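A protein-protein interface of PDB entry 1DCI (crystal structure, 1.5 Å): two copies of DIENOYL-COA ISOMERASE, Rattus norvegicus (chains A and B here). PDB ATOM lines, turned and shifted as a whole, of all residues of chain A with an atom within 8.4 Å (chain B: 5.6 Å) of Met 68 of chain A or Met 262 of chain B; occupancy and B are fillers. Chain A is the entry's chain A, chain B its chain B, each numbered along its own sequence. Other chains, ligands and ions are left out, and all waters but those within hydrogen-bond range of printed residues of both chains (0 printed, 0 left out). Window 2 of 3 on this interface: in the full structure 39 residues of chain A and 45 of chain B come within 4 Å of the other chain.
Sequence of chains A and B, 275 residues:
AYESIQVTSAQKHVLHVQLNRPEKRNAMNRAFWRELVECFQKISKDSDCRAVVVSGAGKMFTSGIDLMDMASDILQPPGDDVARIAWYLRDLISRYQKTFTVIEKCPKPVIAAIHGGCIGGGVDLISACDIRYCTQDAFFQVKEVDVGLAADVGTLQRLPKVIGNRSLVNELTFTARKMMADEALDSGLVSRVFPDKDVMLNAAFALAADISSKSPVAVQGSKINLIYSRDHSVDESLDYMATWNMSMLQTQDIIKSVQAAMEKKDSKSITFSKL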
ATOM      1  N   MET A  28      -3.622  -2.667   9.527  1.00  0.00           N
ATOM      2  CA  MET A  28      -4.340  -3.491   8.579  1.00  0.00           C
ATOM      3  C   MET A  28      -3.938  -3.151   7.148  1.00  0.00           C
ATOM      4  O   MET A  28      -4.473  -2.256   6.503  1.00  0.00           O
ATOM      5  CB  MET A  28      -5.859  -3.352   8.813  1.00  0.00           C
ATOM      6  CG  MET A  28      -6.250  -3.859  10.207  1.00  0.00           C
ATOM      7  SD  MET A  28      -7.970  -3.326  10.534  1.00  0.00           S
ATOM      8  CE  MET A  28      -8.265  -4.201  12.070  1.00  0.00           C
ATOM      9  N   ASN A  29      -2.904  -3.874   6.699  1.00  0.00           N
ATOM     10  CA  ASN A  29      -2.387  -3.645   5.339  1.00  0.00           C
ATOM     11  C   ASN A  29      -3.106  -4.531   4.357  1.00  0.00           C
ATOM     12  O   ASN A  29      -3.967  -5.330   4.736  1.00  0.00           O
ATOM     13  CB  ASN A  29      -0.886  -3.861   5.295  1.00  0.00           C
ATOM     14  CG  ASN A  29      -0.452  -5.262   5.637  1.00  0.00           C
ATOM     15  OD1 ASN A  29      -1.210  -6.062   6.178  1.00  0.00           O
ATOM     16  ND2 ASN A  29       0.800  -5.589   5.311  1.00  0.00           N
ATOM     17  N   ARG A  30      -2.737  -4.482   3.085  1.00  0.00           N
ATOM     18  CA  ARG A  30      -3.468  -5.174   2.040  1.00  0.00           C
ATOM     19  C   ARG A  30      -3.660  -6.660   2.296  1.00  0.00           C
ATOM     20  O   ARG A  30      -4.768  -7.183   2.116  1.00  0.00           O
ATOM     21  CB  ARG A  30      -2.824  -4.901   0.670  1.00  0.00           C
ATOM     22  CG  ARG A  30      -3.737  -5.185  -0.498  1.00  0.00           C
ATOM     23  CD  ARG A  30      -3.131  -4.704  -1.814  1.00  0.00           C
ATOM     24  NE  ARG A  30      -3.008  -3.251  -1.820  1.00  0.00           N
ATOM     25  CZ  ARG A  30      -1.842  -2.602  -1.807  1.00  0.00           C
ATOM     26  NH1 ARG A  30      -0.697  -3.286  -1.748  1.00  0.00           N
ATOM     27  NH2 ARG A  30      -1.811  -1.274  -1.820  1.00  0.00           N
ATOM     28  N   ILE A  65      -6.307   0.863   9.787  1.00  0.00           N
ATOM     29  CA  ILE A  65      -5.901   0.687   8.396  1.00  0.00           C
ATOM     30  C   ILE A  65      -4.547   1.306   8.104  1.00  0.00           C
ATOM     31  O   ILE A  65      -4.155   2.331   8.652  1.00  0.00           O
ATOM     32  CB  ILE A  65      -6.971   1.227   7.419  1.00  0.00           C
ATOM     33  CG1 ILE A  65      -6.739   0.663   6.019  1.00  0.00           C
ATOM     34  CG2 ILE A  65      -6.969   2.749   7.373  1.00  0.00           C
ATOM     35  CD1 ILE A  65      -7.864   0.876   5.032  1.00  0.00           C
ATOM     36  N   ASP A  66      -3.791   0.604   7.255  1.00  0.00           N
ATOM     37  CA  ASP A  66      -2.540   1.143   6.705  1.00  0.00           C
ATOM     38  C   ASP A  66      -2.937   2.222   5.696  1.00  0.00           C
ATOM     39  O   ASP A  66      -3.484   1.926   4.626  1.00  0.00           O
ATOM     40  CB  ASP A  66      -1.787  -0.008   6.060  1.00  0.00           C
ATOM     41  CG  ASP A  66      -0.500   0.401   5.365  1.00  0.00           C
ATOM     42  OD1 ASP A  66      -0.380   1.542   4.881  1.00  0.00           O
ATOM     43  OD2 ASP A  66       0.392  -0.449   5.295  1.00  0.00           O
ATOM     44  N   LEU A  67      -2.649   3.475   6.026  1.00  0.00           N
ATOM     45  CA  LEU A  67      -3.028   4.615   5.194  1.00  0.00           C
ATOM     46  C   LEU A  67      -2.341   4.661   3.837  1.00  0.00           C
ATOM     47  O   LEU A  67      -2.931   5.145   2.868  1.00  0.00           O
ATOM     48  CB  LEU A  67      -2.757   5.907   5.970  1.00  0.00           C
ATOM     49  CG  LEU A  67      -3.898   6.747   6.527  1.00  0.00           C
ATOM     50  CD1 LEU A  67      -5.169   5.958   6.759  1.00  0.00           C
ATOM     51  CD2 LEU A  67      -3.459   7.430   7.821  1.00  0.00           C
ATOM     52  N   MET A  68      -1.107   4.170   3.766  1.00  0.00           N
ATOM     53  CA  MET A  68      -0.364   4.195   2.503  1.00  0.00           C
ATOM     54  C   MET A  68      -0.981   3.197   1.548  1.00  0.00           C
ATOM     55  O   MET A  68      -1.207   3.480   0.376  1.00  0.00           O
ATOM     56  CB  MET A  68       1.117   3.930   2.738  1.00  0.00           C
ATOM     57  CG  MET A  68       1.702   4.894   3.774  1.00  0.00           C
ATOM     58  SD  MET A  68       1.560   6.614   3.209  1.00  0.00           S
ATOM     59  CE  MET A  68       2.978   6.624   2.105  1.00  0.00           C
ATOM     60  N   ASP A  69      -1.295   1.992   2.085  1.00  0.00           N
ATOM     61  CA  ASP A  69      -1.937   1.015   1.208  1.00  0.00           C
ATOM     62  C   ASP A  69      -3.337   1.525   0.810  1.00  0.00           C
ATOM     63  O   ASP A  69      -3.747   1.338  -0.332  1.00  0.00           O
ATOM     64  CB  ASP A  69      -2.093  -0.347   1.886  1.00  0.00           C
ATOM     65  CG  ASP A  69      -0.810  -1.173   1.869  1.00  0.00           C
ATOM     66  OD1 ASP A  69       0.225  -0.716   1.351  1.00  0.00           O
ATOM     67  OD2 ASP A  69      -0.822  -2.307   2.417  1.00  0.00           O
ATOM     68  N   MET A  70      -4.014   2.166   1.773  1.00  0.00           N
ATOM     69  CA  MET A  70      -5.354   2.667   1.463  1.00  0.00           C
ATOM     70  C   MET A  70      -5.295   3.706   0.345  1.00  0.00           C
ATOM     71  O   MET A  70      -6.077   3.592  -0.600  1.00  0.00           O
ATOM     72  CB  MET A  70      -6.002   3.233   2.720  1.00  0.00           C
ATOM     73  CG  MET A  70      -7.478   3.561   2.421  1.00  0.00           C
ATOM     74  SD  MET A  70      -8.084   4.738   3.656  1.00  0.00           S
ATOM     75  CE  MET A  70      -7.253   6.215   3.048  1.00  0.00           C
ATOM     76  N   ALA A  71      -4.357   4.639   0.432  1.00  0.00           N
ATOM     77  CA  ALA A  71      -4.211   5.650  -0.617  1.00  0.00           C
ATOM     78  C   ALA A  71      -3.901   5.000  -1.949  1.00  0.00           C
ATOM     79  O   ALA A  71      -4.532   5.252  -2.982  1.00  0.00           O
ATOM     80  CB  ALA A  71      -3.097   6.620  -0.230  1.00  0.00           C
ATOM     81  N   SER A  72      -2.971   4.019  -1.973  1.00  0.00           N
ATOM     82  CA  SER A  72      -2.718   3.325  -3.232  1.00  0.00           C
ATOM     83  C   SER A  72      -3.996   2.697  -3.775  1.00  0.00           C
ATOM     84  O   SER A  72      -4.268   2.786  -4.970  1.00  0.00           O
ATOM     85  CB  SER A  72      -1.628   2.255  -3.061  1.00  0.00           C
ATOM     86  OG  SER A  72      -1.456   1.559  -4.273  1.00  0.00           O
ATOM     87  N   ASP A  73      -4.774   2.044  -2.903  1.00  0.00           N
ATOM     88  CA  ASP A  73      -5.978   1.371  -3.370  1.00  0.00           C
ATOM     89  C   ASP A  73      -7.090   2.372  -3.740  1.00  0.00           C
ATOM     90  O   ASP A  73      -7.714   2.075  -4.749  1.00  0.00           O
ATOM     91  CB  ASP A  73      -6.530   0.405  -2.333  1.00  0.00           C
ATOM     92  CG  ASP A  73      -5.649  -0.764  -1.936  1.00  0.00           C
ATOM     93  OD1 ASP A  73      -4.745  -1.140  -2.699  1.00  0.00           O
ATOM     94  OD2 ASP A  73      -5.911  -1.334  -0.847  1.00  0.00           O
ATOM     95  N   ILE A  74      -7.190   3.469  -3.036  1.00  0.00           N
ATOM     96  CA  ILE A  74      -8.278   4.434  -3.069  1.00  0.00           C
ATOM     97  C   ILE A  74      -7.951   5.801  -3.627  1.00  0.00           C
ATOM     98  O   ILE A  74      -8.834   6.407  -4.265  1.00  0.00           O
ATOM     99  CB  ILE A  74      -8.855   4.517  -1.631  1.00  0.00           C
ATOM    100  CG1 ILE A  74     -10.000   3.497  -1.524  1.00  0.00           C
ATOM    101  CG2 ILE A  74      -9.315   5.874  -1.164  1.00  0.00           C
ATOM    102  CD1 ILE A  74     -10.015   2.759  -0.200  1.00  0.00           C
ATOM    103  N   LEU A  75      -6.738   6.339  -3.489  1.00  0.00           N
ATOM    104  CA  LEU A  75      -6.374   7.624  -4.067  1.00  0.00           C
ATOM    105  C   LEU A  75      -5.651   7.451  -5.403  1.00  0.00           C
ATOM    106  O   LEU A  75      -5.378   8.421  -6.116  1.00  0.00           O
ATOM    107  CB  LEU A  75      -5.509   8.501  -3.166  1.00  0.00           C
ATOM    108  CG  LEU A  75      -5.889   8.702  -1.705  1.00  0.00           C
ATOM    109  CD1 LEU A  75      -5.142   9.901  -1.122  1.00  0.00           C
ATOM    110  CD2 LEU A  75      -7.383   8.909  -1.508  1.00  0.00           C
ATOM    111  N   GLN A  76      -5.413   6.211  -5.820  1.00  0.00           N
ATOM    112  CA  GLN A  76      -4.801   5.857  -7.083  1.00  0.00           C
ATOM    113  C   GLN A  76      -5.545   4.718  -7.782  1.00  0.00           C
ATOM    114  O   GLN A  76      -5.044   3.615  -8.015  1.00  0.00           O
ATOM    115  CB  GLN A  76      -3.351   5.417  -6.869  1.00  0.00           C
ATOM    116  CG  GLN A  76      -2.319   6.394  -6.371  1.00  0.00           C
ATOM    117  CD  GLN A  76      -1.442   6.967  -7.465  1.00  0.00           C
ATOM    118  OE1 GLN A  76      -0.523   6.288  -7.923  1.00  0.00           O
ATOM    119  NE2 GLN A  76      -1.692   8.200  -7.886  1.00  0.00           N
ATOM    120  N   SER B 257      -6.108  14.380   4.105  1.00  0.00           N
ATOM    121  CA  SER B 257      -5.837  13.726   5.383  1.00  0.00           C
ATOM    122  C   SER B 257      -4.678  12.746   5.301  1.00  0.00           C
ATOM    123  O   SER B 257      -3.883  12.686   6.238  1.00  0.00           O
ATOM    124  CB  SER B 257      -7.094  13.007   5.879  1.00  0.00           C
ATOM    125  OG  SER B 257      -8.226  13.863   5.903  1.00  0.00           O
ATOM    126  N   VAL B 258      -4.545  12.040   4.175  1.00  0.00           N
ATOM    127  CA  VAL B 258      -3.399  11.120   4.052  1.00  0.00           C
ATOM    128  C   VAL B 258      -2.127  11.959   3.948  1.00  0.00           C
ATOM    129  O   VAL B 258      -1.133  11.612   4.594  1.00  0.00           O
ATOM    130  CB  VAL B 258      -3.550  10.144   2.886  1.00  0.00           C
ATOM    131  CG1 VAL B 258      -2.346   9.205   2.796  1.00  0.00           C
ATOM    132  CG2 VAL B 258      -4.820   9.307   3.050  1.00  0.00           C
ATOM    133  N   GLN B 259      -2.169  13.054   3.197  1.00  0.00           N
ATOM    134  CA  GLN B 259      -0.995  13.931   3.086  1.00  0.00           C
ATOM    135  C   GLN B 259      -0.585  14.500   4.433  1.00  0.00           C
ATOM    136  O   GLN B 259       0.613  14.491   4.764  1.00  0.00           O
ATOM    137  CB  GLN B 259      -1.233  15.071   2.092  1.00  0.00           C
ATOM    138  CG  GLN B 259      -1.189  14.581   0.653  1.00  0.00           C
ATOM    139  CD  GLN B 259      -1.624  15.587  -0.381  1.00  0.00           C
ATOM    140  OE1 GLN B 259      -2.189  16.635  -0.045  1.00  0.00           O
ATOM    141  NE2 GLN B 259      -1.393  15.291  -1.656  1.00  0.00           N
ATOM    142  N   ALA B 260      -1.551  14.910   5.263  1.00  0.00           N
ATOM    143  CA  ALA B 260      -1.221  15.398   6.600  1.00  0.00           C
ATOM    144  C   ALA B 260      -0.568  14.305   7.431  1.00  0.00           C
ATOM    145  O   ALA B 260       0.374  14.584   8.181  1.00  0.00           O
ATOM    146  CB  ALA B 260      -2.453  15.938   7.308  1.00  0.00           C
ATOM    147  N   ALA B 261      -1.070  13.073   7.328  1.00  0.00           N
ATOM    148  CA  ALA B 261      -0.515  11.939   8.048  1.00  0.00           C
ATOM    149  C   ALA B 261       0.915  11.654   7.588  1.00  0.00           C
ATOM    150  O   ALA B 261       1.785  11.370   8.406  1.00  0.00           O
ATOM    151  CB  ALA B 261      -1.334  10.667   7.824  1.00  0.00           C
ATOM    152  N   MET B 262       1.152  11.736   6.282  1.00  0.00           N
ATOM    153  CA  MET B 262       2.483  11.520   5.725  1.00  0.00           C
ATOM    154  C   MET B 262       3.512  12.521   6.239  1.00  0.00           C
ATOM    155  O   MET B 262       4.655  12.153   6.542  1.00  0.00           O
ATOM    156  CB  MET B 262       2.418  11.588   4.192  1.00  0.00           C
ATOM    157  CG  MET B 262       1.760  10.360   3.567  1.00  0.00           C
ATOM    158  SD  MET B 262       1.314  10.642   1.842  1.00  0.00           S
ATOM    159  CE  MET B 262       2.946  10.550   1.079  1.00  0.00           C
ATOM    160  N   GLU B 263       3.132  13.792   6.354  1.00  0.00           N
ATOM    161  CA  GLU B 263       4.040  14.829   6.828  1.00  0.00           C
ATOM    162  C   GLU B 263       4.059  14.945   8.346  1.00  0.00           C
ATOM    163  O   GLU B 263       4.918  15.624   8.912  1.00  0.00           O
ATOM    164  CB  GLU B 263       3.676  16.185   6.213  1.00  0.00           C
ATOM    165  CG  GLU B 263       3.402  16.143   4.720  1.00  0.00           C
ATOM    166  CD  GLU B 263       2.502  17.250   4.215  1.00  0.00           C
ATOM    167  OE1 GLU B 263       1.915  18.007   5.019  1.00  0.00           O
ATOM    168  OE2 GLU B 263       2.349  17.376   2.978  1.00  0.00           O
ATOM    169  N   LYS B 264       3.121  14.304   9.028  1.00  0.00           N
ATOM    170  CA  LYS B 264       2.988  14.348  10.473  1.00  0.00           C
ATOM    171  C   LYS B 264       2.324  15.655  10.902  1.00  0.00           C
ATOM    172  O   LYS B 264       2.629  16.250  11.936  1.00  0.00           O
ATOM    173  CB  LYS B 264       4.323  14.144  11.189  1.00  0.00           C
ATOM    174  CG  LYS B 264       4.357  12.905  12.072  1.00  0.00           C
ATOM    175  CD  LYS B 264       4.513  11.641  11.238  1.00  0.00           C
ATOM    176  CE  LYS B 264       3.958  10.425  11.959  1.00  0.00           C
ATOM    177  NZ  LYS B 264       2.567  10.117  11.514  1.00  0.00           N
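Of the 15 printed residues of chain A, 3 touch a printed residue of chain B.
Of the 8 printed residues of chain B, 3 touch a printed residue of chain A.
Hydrophobic or aromatic side chains of chain B within 4 Å of the printed part of chain A: Val 258, Ala 261 and Met 262.
Along chain B the printed residues that touch a printed residue of chain A span positions 258 to 262.
Among the printed residues, 3 pairs touch across the chains.
Among the printed residues, no Asp or Glu carboxylate lies within 4 Å of a Lys or Arg side-chain nitrogen of the other chain.
No position is printed for both chains.
Asn 29 of chain A touches none of the printed residues of chain B.
Ile 65 of chain A touches none of the printed residues of chain B.
Printed residues of chain B within 4 Å of Leu 67 of chain A: Ala 261 (3.9 Å).
Met 68 of chain A touches just one residue of chain B: Met 262 (3.8 Å).
Of the printed residues of chain B, Met 70 of chain A touches Val 258 (3.9 Å).
Of the printed residues of chain A, Val 258 of chain B touches Met 70 (3.9 Å).
Of chain A, only Met 68 comes within 4 Å of Met 262 of chain B.
The nearest residue of chain B that does not touch Met 68 of chain A is Val 258 of chain B (4.7 Å).
The nearest residue of chain A that does not touch Met 262 of chain B is Ala 71 of chain A (6.3 Å).
The backbone carbonyl oxygen (O) of Ala 261 of chain B sits at hydrogen-bond distance from the side-chain amino group (NZ) of Lys 264 of chain B.
The side-chain carboxylate (OD1) of Asp 66 of chain A is in hydrogen-bond range of the backbone NH (N) of Met 68 of chain A, at 2.9 Å.
Leu 67 of chain A touches Ala 261 of chain B.
Met 68 of chain A touches Met 262 of chain B.
CG2 of Val 258 of chain B touches CE of Met 70 of chain A (3.9 Å).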
